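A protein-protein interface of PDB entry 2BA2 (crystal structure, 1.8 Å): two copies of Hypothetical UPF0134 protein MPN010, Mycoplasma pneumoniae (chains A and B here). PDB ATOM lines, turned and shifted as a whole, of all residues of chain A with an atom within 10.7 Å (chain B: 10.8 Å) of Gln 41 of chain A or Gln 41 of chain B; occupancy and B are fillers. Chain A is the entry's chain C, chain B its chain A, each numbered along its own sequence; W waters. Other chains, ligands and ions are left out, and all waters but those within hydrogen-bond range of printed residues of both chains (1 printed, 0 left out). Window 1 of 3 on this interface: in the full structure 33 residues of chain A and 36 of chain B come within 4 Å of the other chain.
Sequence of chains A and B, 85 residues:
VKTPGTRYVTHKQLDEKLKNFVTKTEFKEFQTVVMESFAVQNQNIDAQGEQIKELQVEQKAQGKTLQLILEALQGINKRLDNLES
Water W1 lies within hydrogen-bond range of the side-chain amide oxygen of Gln 48 of chain A and the side-chain amide oxygen of Gln 48 of chain B.
No residue of chain B comes within 4 Å of Ala 39 of chain A. No residue of chain B comes within 4 Å of Val 40 of chain A. Of chain B, only Phe 38, Gln 41, Asn 42 and Ile 45 come within 4 Å of Gln 41 of chain A. No residue of chain B comes within 4 Å of Asn 44 of chain A. Printed residues of chain A within 4 Å of Val 34 of chain B: Val 34 (3.99 Å). No residue of chain A comes within 4 Å of Ser 37 of chain B. No residue of chain A comes within 4 Å of Ala 39 of chain B. No residue of chain A comes within 4 Å of Val 40 of chain B. Gln 41 of chain B touches just one residue of chain A: Gln 41. Of chain A, only Gln 41 (2.8 Å) comes within 4 Å of Asn 42 of chain B. No residue of chain A comes within 4 Å of Asn 44 of chain B. Ile 45 of chain B touches just these residues of chain A: Gln 41, Ile 45 and Gln 48. Of the printed residues of chain A, Gln 48 of chain B touches Gln 48. Glu 50 of chain B touches none of the printed residues of chain A. The nearest residue of chain B that does not touch Gln 41 of chain A is Ala 39 of chain B (5.0 Å). The nearest residue of chain A that does not touch Gln 41 of chain B is Ile 45 of chain A (5.8 Å).
The backbone carbonyl oxygen of Phe 38 of chain B lies within hydrogen-bond range of the side-chain amide nitrogen of Asn 42 of chain B (3.3 Å). The side-chain amide nitrogen (NE2) of Gln 41 of chain B lies close to the side-chain amide nitrogen (ND2) of Asn 44 of chain B (3.2 Å). O of Val 33 of chain A sits at hydrogen-bond distance from OG of Ser 37 of chain A (2.7 Å). ND2 of Asn 42 of chain A lies close to O of Phe 38 of chain A (3.3 Å).
Val 34 of chain A touches Phe 38 of chain B, but with the chains exchanged Phe 38 of chain A does not touch Val 34 of chain B (5.9 Å). Ser 37 of chain A touches Phe 38 of chain B, but with the chains exchanged Phe 38 of chain A does not touch Ser 37 of chain B (7.5 Å). Gln 41 of chain A touches Phe 38 of chain B, but with the chains exchanged Phe 38 of chain A does not touch Gln 41 of chain B (6.6 Å). Gln 41 of chain A touches Ile 45 of chain B, but with the chains exchanged Ile 45 of chain A does not touch Gln 41 of chain B (5.8 Å).
The side-chain amide nitrogen (NE2) of Gln 41 of chain A lies within hydrogen-bond range of the backbone carbonyl oxygen (O) of Phe 38 of chain B (3.0 Å). The side-chain amide oxygen (OD1) of Asn 42 of chain B is in hydrogen-bond range of the side-chain amide nitrogen (NE2) of Gln 41 of chain A (2.8 Å). NE2 of Gln 48 of chain A sits at hydrogen-bond distance from O of Ile 45 of chain B (2.9 Å).
Printed residues of chain B that touch a printed residue of chain A: Val 34, Met 35, Phe 38, Gln 41, Asn 42, Ile 45, Gln 48 and Gly 49. Hydrophobic or aromatic side chains of chain B that line the printed part of chain A: Val 34, Met 35, Phe 38 and Ile 45. Of the 17 printed residues of chain A, 7 touch a printed residue of chain B. Along chain A the printed residues that touch a printed residue of chain B span positions 33 to 48. Among the printed residues, 13 pairs touch across the chains.
Among the printed residues, merely in contact across the chains: Ser 37 of chain A with Phe 38 of chain B, Gln 48 of chain A with Gly 49 of chain B, Gln 41 of chain A with Gln 41 of chain B, Val 34 of chain A with Phe 38 of chain B, Gln 48 of chain A with Gln 48 of chain B, Ile 45 of chain A with Ile 45 of chain B, Gln 41 of chain A with Ile 45 of chain B, Phe 38 of chain A with Phe 38 of chain B, Val 33 of chain A with Met 35 of chain B and Val 34 of chain A with Val 34 of chain B.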
ATOM      1  N   VAL A  33     -17.668   3.929   1.450  1.00  0.00           N
ATOM      2  CA  VAL A  33     -16.365   4.544   1.708  1.00  0.00           C
ATOM      3  C   VAL A  33     -16.086   4.543   3.213  1.00  0.00           C
ATOM      4  O   VAL A  33     -14.961   4.297   3.653  1.00  0.00           O
ATOM      5  CB  VAL A  33     -16.332   6.013   1.216  1.00  0.00           C
ATOM      6  CG1 VAL A  33     -15.028   6.687   1.649  1.00  0.00           C
ATOM      7  CG2 VAL A  33     -16.474   6.060  -0.296  1.00  0.00           C
ATOM      8  N   VAL A  34     -17.117   4.836   3.999  1.00  0.00           N
ATOM      9  CA  VAL A  34     -16.979   4.868   5.452  1.00  0.00           C
ATOM     10  C   VAL A  34     -16.762   3.459   6.015  1.00  0.00           C
ATOM     11  O   VAL A  34     -15.885   3.238   6.851  1.00  0.00           O
ATOM     12  CB  VAL A  34     -18.233   5.489   6.104  1.00  0.00           C
ATOM     13  CG1 VAL A  34     -18.150   5.372   7.622  1.00  0.00           C
ATOM     14  CG2 VAL A  34     -18.360   6.956   5.703  1.00  0.00           C
ATOM     15  N   MET A  35     -17.571   2.509   5.558  1.00  0.00           N
ATOM     16  CA  MET A  35     -17.456   1.136   6.038  1.00  0.00           C
ATOM     17  C   MET A  35     -16.112   0.521   5.682  1.00  0.00           C
ATOM     18  O   MET A  35     -15.541  -0.236   6.469  1.00  0.00           O
ATOM     19  CB  MET A  35     -18.587   0.283   5.470  1.00  0.00           C
ATOM     20  CG  MET A  35     -19.961   0.711   5.956  1.00  0.00           C
ATOM     21  SD  MET A  35     -20.026   0.896   7.753  1.00  0.00           S
ATOM     22  CE  MET A  35     -20.409  -0.790   8.249  1.00  0.00           C
ATOM     23  N   GLU A  36     -15.609   0.829   4.491  1.00  0.00           N
ATOM     24  CA  GLU A  36     -14.319   0.298   4.082  1.00  0.00           C
ATOM     25  C   GLU A  36     -13.234   0.981   4.908  1.00  0.00           C
ATOM     26  O   GLU A  36     -12.228   0.368   5.252  1.00  0.00           O
ATOM     27  CB  GLU A  36     -14.075   0.547   2.592  1.00  0.00           C
ATOM     28  CG  GLU A  36     -12.756  -0.033   2.093  1.00  0.00           C
ATOM     29  CD  GLU A  36     -12.635  -0.005   0.584  1.00  0.00           C
ATOM     30  OE1 GLU A  36     -13.483  -0.626  -0.091  1.00  0.00           O
ATOM     31  OE2 GLU A  36     -11.692   0.634   0.071  1.00  0.00           O
ATOM     32  N   SER A  37     -13.442   2.258   5.222  1.00  0.00           N
ATOM     33  CA  SER A  37     -12.480   3.004   6.024  1.00  0.00           C
ATOM     34  C   SER A  37     -12.362   2.392   7.415  1.00  0.00           C
ATOM     35  O   SER A  37     -11.263   2.155   7.908  1.00  0.00           O
ATOM     36  CB  SER A  37     -12.899   4.472   6.128  1.00  0.00           C
ATOM     37  OG  SER A  37     -12.749   5.124   4.878  1.00  0.00           O
ATOM     38  N   PHE A  38     -13.497   2.136   8.053  1.00  0.00           N
ATOM     39  CA  PHE A  38     -13.468   1.529   9.375  1.00  0.00           C
ATOM     40  C   PHE A  38     -12.796   0.170   9.284  1.00  0.00           C
ATOM     41  O   PHE A  38     -12.020  -0.201  10.158  1.00  0.00           O
ATOM     42  CB  PHE A  38     -14.884   1.360   9.928  1.00  0.00           C
ATOM     43  CG  PHE A  38     -15.398   2.564  10.660  1.00  0.00           C
ATOM     44  CD1 PHE A  38     -16.552   3.215  10.236  1.00  0.00           C
ATOM     45  CD2 PHE A  38     -14.726   3.048  11.781  1.00  0.00           C
ATOM     46  CE1 PHE A  38     -17.034   4.333  10.914  1.00  0.00           C
ATOM     47  CE2 PHE A  38     -15.199   4.165  12.469  1.00  0.00           C
ATOM     48  CZ  PHE A  38     -16.353   4.808  12.034  1.00  0.00           C
ATOM     49  N   ALA A  39     -13.098  -0.567   8.215  1.00  0.00           N
ATOM     50  CA  ALA A  39     -12.533  -1.904   8.023  1.00  0.00           C
ATOM     51  C   ALA A  39     -11.007  -1.905   8.011  1.00  0.00           C
ATOM     52  O   ALA A  39     -10.370  -2.697   8.705  1.00  0.00           O
ATOM     53  CB  ALA A  39     -13.069  -2.510   6.729  1.00  0.00           C
ATOM     54  N   VAL A  40     -10.422  -1.011   7.227  1.00  0.00           N
ATOM     55  CA  VAL A  40      -8.972  -0.923   7.134  1.00  0.00           C
ATOM     56  C   VAL A  40      -8.314  -0.443   8.430  1.00  0.00           C
ATOM     57  O   VAL A  40      -7.291  -0.987   8.848  1.00  0.00           O
ATOM     58  CB  VAL A  40      -8.564  -0.005   5.964  1.00  0.00           C
ATOM     59  CG1 VAL A  40      -7.053   0.196   5.951  1.00  0.00           C
ATOM     60  CG2 VAL A  40      -9.029  -0.631   4.648  1.00  0.00           C
ATOM     61  N   GLN A  41      -8.893   0.572   9.069  1.00  0.00           N
ATOM     62  CA  GLN A  41      -8.324   1.071  10.313  1.00  0.00           C
ATOM     63  C   GLN A  41      -8.449   0.023  11.417  1.00  0.00           C
ATOM     64  O   GLN A  41      -7.498  -0.221  12.155  1.00  0.00           O
ATOM     65  CB  GLN A  41      -9.014   2.369  10.762  1.00  0.00           C
ATOM     66  CG  GLN A  41      -8.849   3.550   9.814  1.00  0.00           C
ATOM     67  CD  GLN A  41      -9.172   4.883  10.477  1.00  0.00           C
ATOM     68  OE1 GLN A  41     -10.040   4.965  11.354  1.00  0.00           O
ATOM     69  NE2 GLN A  41      -8.480   5.941  10.048  1.00  0.00           N
ATOM     70  N   ASN A  42      -9.622  -0.594  11.522  1.00  0.00           N
ATOM     71  CA  ASN A  42      -9.868  -1.608  12.545  1.00  0.00           C
ATOM     72  C   ASN A  42      -8.996  -2.832  12.357  1.00  0.00           C
ATOM     73  O   ASN A  42      -8.653  -3.527  13.321  1.00  0.00           O
ATOM     74  CB  ASN A  42     -11.344  -2.002  12.560  1.00  0.00           C
ATOM     75  CG  ASN A  42     -12.226  -0.895  13.107  1.00  0.00           C
ATOM     76  OD1 ASN A  42     -11.731   0.068  13.697  1.00  0.00           O
ATOM     77  ND2 ASN A  42     -13.531  -1.028  12.926  1.00  0.00           N
ATOM     78  N   GLN A  43      -8.628  -3.091  11.111  1.00  0.00           N
ATOM     79  CA  GLN A  43      -7.756  -4.210  10.801  1.00  0.00           C
ATOM     80  C   GLN A  43      -6.363  -3.843  11.313  1.00  0.00           C
ATOM     81  O   GLN A  43      -5.622  -4.691  11.801  1.00  0.00           O
ATOM     82  CB  GLN A  43      -7.708  -4.441   9.291  1.00  0.00           C
ATOM     83  CG  GLN A  43      -7.301  -5.851   8.907  1.00  0.00           C
ATOM     84  CD  GLN A  43      -6.166  -5.880   7.912  1.00  0.00           C
ATOM     85  OE1 GLN A  43      -5.065  -5.406   8.200  1.00  0.00           O
ATOM     86  NE2 GLN A  43      -6.421  -6.438   6.733  1.00  0.00           N
ATOM     87  N   ASN A  44      -6.011  -2.568  11.194  1.00  0.00           N
ATOM     88  CA  ASN A  44      -4.712  -2.101  11.668  1.00  0.00           C
ATOM     89  C   ASN A  44      -4.717  -2.140  13.186  1.00  0.00           C
ATOM     90  O   ASN A  44      -3.763  -2.593  13.810  1.00  0.00           O
ATOM     91  CB  ASN A  44      -4.448  -0.668  11.193  1.00  0.00           C
ATOM     92  CG  ASN A  44      -4.017  -0.604   9.743  1.00  0.00           C
ATOM     93  OD1 ASN A  44      -4.692  -1.125   8.855  1.00  0.00           O
ATOM     94  ND2 ASN A  44      -2.883   0.040   9.496  1.00  0.00           N
ATOM     95  N   ILE A  45      -5.809  -1.674  13.781  1.00  0.00           N
ATOM     96  CA  ILE A  45      -5.916  -1.668  15.231  1.00  0.00           C
ATOM     97  C   ILE A  45      -5.826  -3.091  15.796  1.00  0.00           C
ATOM     98  O   ILE A  45      -5.172  -3.323  16.817  1.00  0.00           O
ATOM     99  CB  ILE A  45      -7.232  -0.998  15.682  1.00  0.00           C
ATOM    100  CG1 ILE A  45      -7.203   0.492  15.313  1.00  0.00           C
ATOM    101  CG2 ILE A  45      -7.412  -1.157  17.187  1.00  0.00           C
ATOM    102  CD1 ILE A  45      -8.522   1.220  15.545  1.00  0.00           C
ATOM    103  N   ASP A  46      -6.465  -4.042  15.124  1.00  0.00           N
ATOM    104  CA  ASP A  46      -6.435  -5.431  15.571  1.00  0.00           C
ATOM    105  C   ASP A  46      -5.038  -6.033  15.417  1.00  0.00           C
ATOM    106  O   ASP A  46      -4.584  -6.798  16.275  1.00  0.00           O
ATOM    107  CB  ASP A  46      -7.458  -6.271  14.794  1.00  0.00           C
ATOM    108  CG  ASP A  46      -8.888  -5.995  15.227  1.00  0.00           C
ATOM    109  OD1 ASP A  46      -9.134  -5.901  16.449  1.00  0.00           O
ATOM    110  OD2 ASP A  46      -9.770  -5.883  14.349  1.00  0.00           O
ATOM    111  N   ALA A  47      -4.355  -5.677  14.334  1.00  0.00           N
ATOM    112  CA  ALA A  47      -3.009  -6.177  14.092  1.00  0.00           C
ATOM    113  C   ALA A  47      -2.078  -5.684  15.193  1.00  0.00           C
ATOM    114  O   ALA A  47      -1.226  -6.425  15.677  1.00  0.00           O
ATOM    115  CB  ALA A  47      -2.509  -5.712  12.732  1.00  0.00           C
ATOM    116  N   GLN A  48      -2.245  -4.427  15.592  1.00  0.00           N
ATOM    117  CA  GLN A  48      -1.415  -3.854  16.649  1.00  0.00           C
ATOM    118  C   GLN A  48      -1.736  -4.497  17.997  1.00  0.00           C
ATOM    119  O   GLN A  48      -0.852  -4.681  18.824  1.00  0.00           O
ATOM    120  CB  GLN A  48      -1.622  -2.334  16.717  1.00  0.00           C
ATOM    121  CG  GLN A  48      -0.943  -1.588  15.572  1.00  0.00           C
ATOM    122  CD  GLN A  48      -1.221  -0.088  15.581  1.00  0.00           C
ATOM    123  OE1 GLN A  48      -1.700   0.463  16.568  1.00  0.00           O
ATOM    124  NE2 GLN A  48      -0.903   0.574  14.478  1.00  0.00           N
ATOM    125  N   GLY A  49      -3.005  -4.833  18.214  1.00  0.00           N
ATOM    126  CA  GLY A  49      -3.380  -5.474  19.465  1.00  0.00           C
ATOM    127  C   GLY A  49      -2.681  -6.818  19.549  1.00  0.00           C
ATOM    128  O   GLY A  49      -2.257  -7.255  20.620  1.00  0.00           O
ATOM    129  N   THR B  32     -17.582  15.615   5.714  1.00  0.00           N
ATOM    130  CA  THR B  32     -16.335  16.266   6.093  1.00  0.00           C
ATOM    131  C   THR B  32     -15.865  15.872   7.487  1.00  0.00           C
ATOM    132  O   THR B  32     -14.709  15.503   7.670  1.00  0.00           O
ATOM    133  CB  THR B  32     -16.467  17.803   6.015  1.00  0.00           C
ATOM    134  OG1 THR B  32     -17.438  18.254   6.964  1.00  0.00           O
ATOM    135  CG2 THR B  32     -16.900  18.220   4.632  1.00  0.00           C
ATOM    136  N   VAL B  33     -16.759  15.959   8.470  1.00  0.00           N
ATOM    137  CA  VAL B  33     -16.413  15.602   9.843  1.00  0.00           C
ATOM    138  C   VAL B  33     -15.976  14.140   9.924  1.00  0.00           C
ATOM    139  O   VAL B  33     -15.046  13.799  10.651  1.00  0.00           O
ATOM    140  CB  VAL B  33     -17.611  15.821  10.800  1.00  0.00           C
ATOM    141  CG1 VAL B  33     -17.225  15.442  12.217  1.00  0.00           C
ATOM    142  CG2 VAL B  33     -18.052  17.262  10.754  1.00  0.00           C
ATOM    143  N   VAL B  34     -16.650  13.274   9.173  1.00  0.00           N
ATOM    144  CA  VAL B  34     -16.294  11.863   9.186  1.00  0.00           C
ATOM    145  C   VAL B  34     -14.924  11.623   8.545  1.00  0.00           C
ATOM    146  O   VAL B  34     -14.084  10.965   9.126  1.00  0.00           O
ATOM    147  CB  VAL B  34     -17.337  11.012   8.437  1.00  0.00           C
ATOM    148  CG1 VAL B  34     -16.829   9.584   8.279  1.00  0.00           C
ATOM    149  CG2 VAL B  34     -18.655  11.008   9.206  1.00  0.00           C
ATOM    150  N   MET B  35     -14.696  12.150   7.346  1.00  0.00           N
ATOM    151  CA  MET B  35     -13.416  11.919   6.681  1.00  0.00           C
ATOM    152  C   MET B  35     -12.287  12.560   7.471  1.00  0.00           C
ATOM    153  O   MET B  35     -11.178  12.021   7.580  1.00  0.00           O
ATOM    154  CB  MET B  35     -13.461  12.461   5.246  1.00  0.00           C
ATOM    155  CG  MET B  35     -14.447  11.699   4.346  1.00  0.00           C
ATOM    156  SD  MET B  35     -14.390   9.879   4.568  1.00  0.00           S
ATOM    157  CE  MET B  35     -13.064   9.470   3.469  1.00  0.00           C
ATOM    158  N   GLU B  36     -12.586  13.715   8.040  1.00  0.00           N
ATOM    159  CA  GLU B  36     -11.613  14.430   8.832  1.00  0.00           C
ATOM    160  C   GLU B  36     -11.321  13.654  10.122  1.00  0.00           C
ATOM    161  O   GLU B  36     -10.187  13.638  10.608  1.00  0.00           O
ATOM    162  CB  GLU B  36     -12.141  15.842   9.088  1.00  0.00           C
ATOM    163  CG  GLU B  36     -11.797  16.789   7.946  1.00  0.00           C
ATOM    164  CD  GLU B  36     -12.284  18.206   8.159  1.00  0.00           C
ATOM    165  OE1 GLU B  36     -12.671  18.556   9.294  1.00  0.00           O
ATOM    166  OE2 GLU B  36     -12.268  18.976   7.180  1.00  0.00           O
ATOM    167  N   SER B  37     -12.335  12.987  10.670  1.00  0.00           N
ATOM    168  CA  SER B  37     -12.138  12.197  11.877  1.00  0.00           C
ATOM    169  C   SER B  37     -11.287  10.961  11.567  1.00  0.00           C
ATOM    170  O   SER B  37     -10.506  10.506  12.404  1.00  0.00           O
ATOM    171  CB  SER B  37     -13.482  11.757  12.466  1.00  0.00           C
ATOM    172  OG  SER B  37     -14.195  12.865  12.984  1.00  0.00           O
ATOM    173  N   PHE B  38     -11.444  10.403  10.370  1.00  0.00           N
ATOM    174  CA  PHE B  38     -10.647   9.241   9.998  1.00  0.00           C
ATOM    175  C   PHE B  38      -9.194   9.673   9.928  1.00  0.00           C
ATOM    176  O   PHE B  38      -8.308   8.920  10.305  1.00  0.00           O
ATOM    177  CB  PHE B  38     -11.071   8.690   8.634  1.00  0.00           C
ATOM    178  CG  PHE B  38     -12.242   7.743   8.691  1.00  0.00           C
ATOM    179  CD1 PHE B  38     -13.343   7.932   7.862  1.00  0.00           C
ATOM    180  CD2 PHE B  38     -12.227   6.647   9.549  1.00  0.00           C
ATOM    181  CE1 PHE B  38     -14.423   7.037   7.883  1.00  0.00           C
ATOM    182  CE2 PHE B  38     -13.301   5.748   9.577  1.00  0.00           C
ATOM    183  CZ  PHE B  38     -14.397   5.945   8.743  1.00  0.00           C
ATOM    184  N   ALA B  39      -8.957  10.891   9.443  1.00  0.00           N
ATOM    185  CA  ALA B  39      -7.591  11.413   9.326  1.00  0.00           C
ATOM    186  C   ALA B  39      -6.952  11.463  10.705  1.00  0.00           C
ATOM    187  O   ALA B  39      -5.809  11.052  10.883  1.00  0.00           O
ATOM    188  CB  ALA B  39      -7.606  12.806   8.708  1.00  0.00           C
ATOM    189  N   VAL B  40      -7.699  11.972  11.678  1.00  0.00           N
ATOM    190  CA  VAL B  40      -7.209  12.052  13.047  1.00  0.00           C
ATOM    191  C   VAL B  40      -6.877  10.646  13.560  1.00  0.00           C
ATOM    192  O   VAL B  40      -5.821  10.426  14.159  1.00  0.00           O
ATOM    193  CB  VAL B  40      -8.265  12.713  13.963  1.00  0.00           C
ATOM    194  CG1 VAL B  40      -7.804  12.681  15.415  1.00  0.00           C
ATOM    195  CG2 VAL B  40      -8.491  14.145  13.526  1.00  0.00           C
ATOM    196  N   GLN B  41      -7.774   9.693  13.313  1.00  0.00           N
ATOM    197  CA  GLN B  41      -7.550   8.317  13.760  1.00  0.00           C
ATOM    198  C   GLN B  41      -6.308   7.724  13.104  1.00  0.00           C
ATOM    199  O   GLN B  41      -5.576   6.976  13.736  1.00  0.00           O
ATOM    200  CB  GLN B  41      -8.770   7.445  13.446  1.00  0.00           C
ATOM    201  CG  GLN B  41     -10.021   7.842  14.210  1.00  0.00           C
ATOM    202  CD  GLN B  41      -9.884   7.628  15.708  1.00  0.00           C
ATOM    203  OE1 GLN B  41     -10.416   6.663  16.262  1.00  0.00           O
ATOM    204  NE2 GLN B  41      -9.160   8.524  16.368  1.00  0.00           N
ATOM    205  N   ASN B  42      -6.074   8.051  11.834  1.00  0.00           N
ATOM    206  CA  ASN B  42      -4.886   7.542  11.151  1.00  0.00           C
ATOM    207  C   ASN B  42      -3.642   7.995  11.910  1.00  0.00           C
ATOM    208  O   ASN B  42      -2.694   7.233  12.087  1.00  0.00           O
ATOM    209  CB  ASN B  42      -4.803   8.056   9.709  1.00  0.00           C
ATOM    210  CG  ASN B  42      -5.743   7.328   8.770  1.00  0.00           C
ATOM    211  OD1 ASN B  42      -5.953   6.118   8.899  1.00  0.00           O
ATOM    212  ND2 ASN B  42      -6.297   8.056   7.797  1.00  0.00           N
ATOM    213  N   GLN B  43      -3.658   9.244  12.359  1.00  0.00           N
ATOM    214  CA  GLN B  43      -2.538   9.798  13.103  1.00  0.00           C
ATOM    215  C   GLN B  43      -2.351   9.040  14.414  1.00  0.00           C
ATOM    216  O   GLN B  43      -1.232   8.700  14.785  1.00  0.00           O
ATOM    217  CB  GLN B  43      -2.788  11.272  13.401  1.00  0.00           C
ATOM    218  CG  GLN B  43      -1.522  12.099  13.541  1.00  0.00           C
ATOM    219  CD  GLN B  43      -0.862  12.408  12.210  1.00  0.00           C
ATOM    220  OE1 GLN B  43      -0.368  11.511  11.530  1.00  0.00           O
ATOM    221  NE2 GLN B  43      -0.856  13.683  11.830  1.00  0.00           N
ATOM    222  N   ASN B  44      -3.457   8.781  15.109  1.00  0.00           N
ATOM    223  CA  ASN B  44      -3.406   8.069  16.380  1.00  0.00           C
ATOM    224  C   ASN B  44      -2.954   6.623  16.222  1.00  0.00           C
ATOM    225  O   ASN B  44      -2.103   6.150  16.967  1.00  0.00           O
ATOM    226  CB  ASN B  44      -4.773   8.090  17.067  1.00  0.00           C
ATOM    227  CG  ASN B  44      -5.180   9.478  17.514  1.00  0.00           C
ATOM    228  OD1 ASN B  44      -4.331  10.311  17.832  1.00  0.00           O
ATOM    229  ND2 ASN B  44      -6.492   9.727  17.561  1.00  0.00           N
ATOM    230  N   ILE B  45      -3.531   5.922  15.256  1.00  0.00           N
ATOM    231  CA  ILE B  45      -3.180   4.525  15.025  1.00  0.00           C
ATOM    232  C   ILE B  45      -1.723   4.365  14.598  1.00  0.00           C
ATOM    233  O   ILE B  45      -1.020   3.452  15.050  1.00  0.00           O
ATOM    234  CB  ILE B  45      -4.097   3.905  13.947  1.00  0.00           C
ATOM    235  CG1 ILE B  45      -5.557   4.000  14.402  1.00  0.00           C
ATOM    236  CG2 ILE B  45      -3.714   2.451  13.703  1.00  0.00           C
ATOM    237  CD1 ILE B  45      -6.565   3.593  13.336  1.00  0.00           C
ATOM    238  N   ASP B  46      -1.258   5.259  13.734  1.00  0.00           N
ATOM    239  CA  ASP B  46       0.123   5.173  13.269  1.00  0.00           C
ATOM    240  C   ASP B  46       1.100   5.473  14.399  1.00  0.00           C
ATOM    241  O   ASP B  46       2.177   4.878  14.481  1.00  0.00           O
ATOM    242  CB  ASP B  46       0.366   6.146  12.113  1.00  0.00           C
ATOM    243  CG  ASP B  46       1.740   5.968  11.486  1.00  0.00           C
ATOM    244  OD1 ASP B  46       2.555   6.907  11.545  1.00  0.00           O
ATOM    245  OD2 ASP B  46       2.004   4.875  10.942  1.00  0.00           O
ATOM    246  N   ALA B  47       0.719   6.403  15.267  1.00  0.00           N
ATOM    247  CA  ALA B  47       1.558   6.785  16.395  1.00  0.00           C
ATOM    248  C   ALA B  47       1.751   5.584  17.315  1.00  0.00           C
ATOM    249  O   ALA B  47       2.856   5.329  17.804  1.00  0.00           O
ATOM    250  CB  ALA B  47       0.910   7.946  17.160  1.00  0.00           C
ATOM    251  N   GLN B  48       0.676   4.841  17.557  1.00  0.00           N
ATOM    252  CA  GLN B  48       0.793   3.667  18.404  1.00  0.00           C
ATOM    253  C   GLN B  48       1.598   2.599  17.668  1.00  0.00           C
ATOM    254  O   GLN B  48       2.321   1.829  18.284  1.00  0.00           O
ATOM    255  CB  GLN B  48      -0.586   3.114  18.782  1.00  0.00           C
ATOM    256  CG  GLN B  48      -1.453   4.071  19.591  1.00  0.00           C
ATOM    257  CD  GLN B  48      -2.588   3.347  20.308  1.00  0.00           C
ATOM    258  OE1 GLN B  48      -3.256   2.499  19.725  1.00  0.00           O
ATOM    259  NE2 GLN B  48      -2.809   3.687  21.572  1.00  0.00           N
ATOM    260  N   GLY B  49       1.462   2.547  16.346  1.00  0.00           N
ATOM    261  CA  GLY B  49       2.213   1.565  15.586  1.00  0.00           C
ATOM    262  C   GLY B  49       3.705   1.779  15.782  1.00  0.00           C
ATOM    263  O   GLY B  49       4.479   0.824  15.898  1.00  0.00           O
ATOM    264  N   GLU B  50       4.097   3.050  15.834  1.00  0.00           N
ATOM    265  CA  GLU B  50       5.489   3.457  16.018  1.00  0.00           C
ATOM    266  C   GLU B  50       5.937   3.145  17.446  1.00  0.00           C
ATOM    267  O   GLU B  50       7.089   2.782  17.679  1.00  0.00           O
ATOM    268  CB  GLU B  50       5.625   4.958  15.740  1.00  0.00           C
ATOM    269  CG  GLU B  50       7.052   5.476  15.703  1.00  0.00           C
ATOM    270  CD  GLU B  50       7.131   6.960  15.370  1.00  0.00           C
ATOM    271  OE1 GLU B  50       8.254   7.471  15.174  1.00  0.00           O
ATOM    272  OE2 GLU B  50       6.069   7.618  15.309  1.00  0.00           O
HETATM  273  O   HOH W   1      -3.937   1.308  17.353  1.00  0.00           O
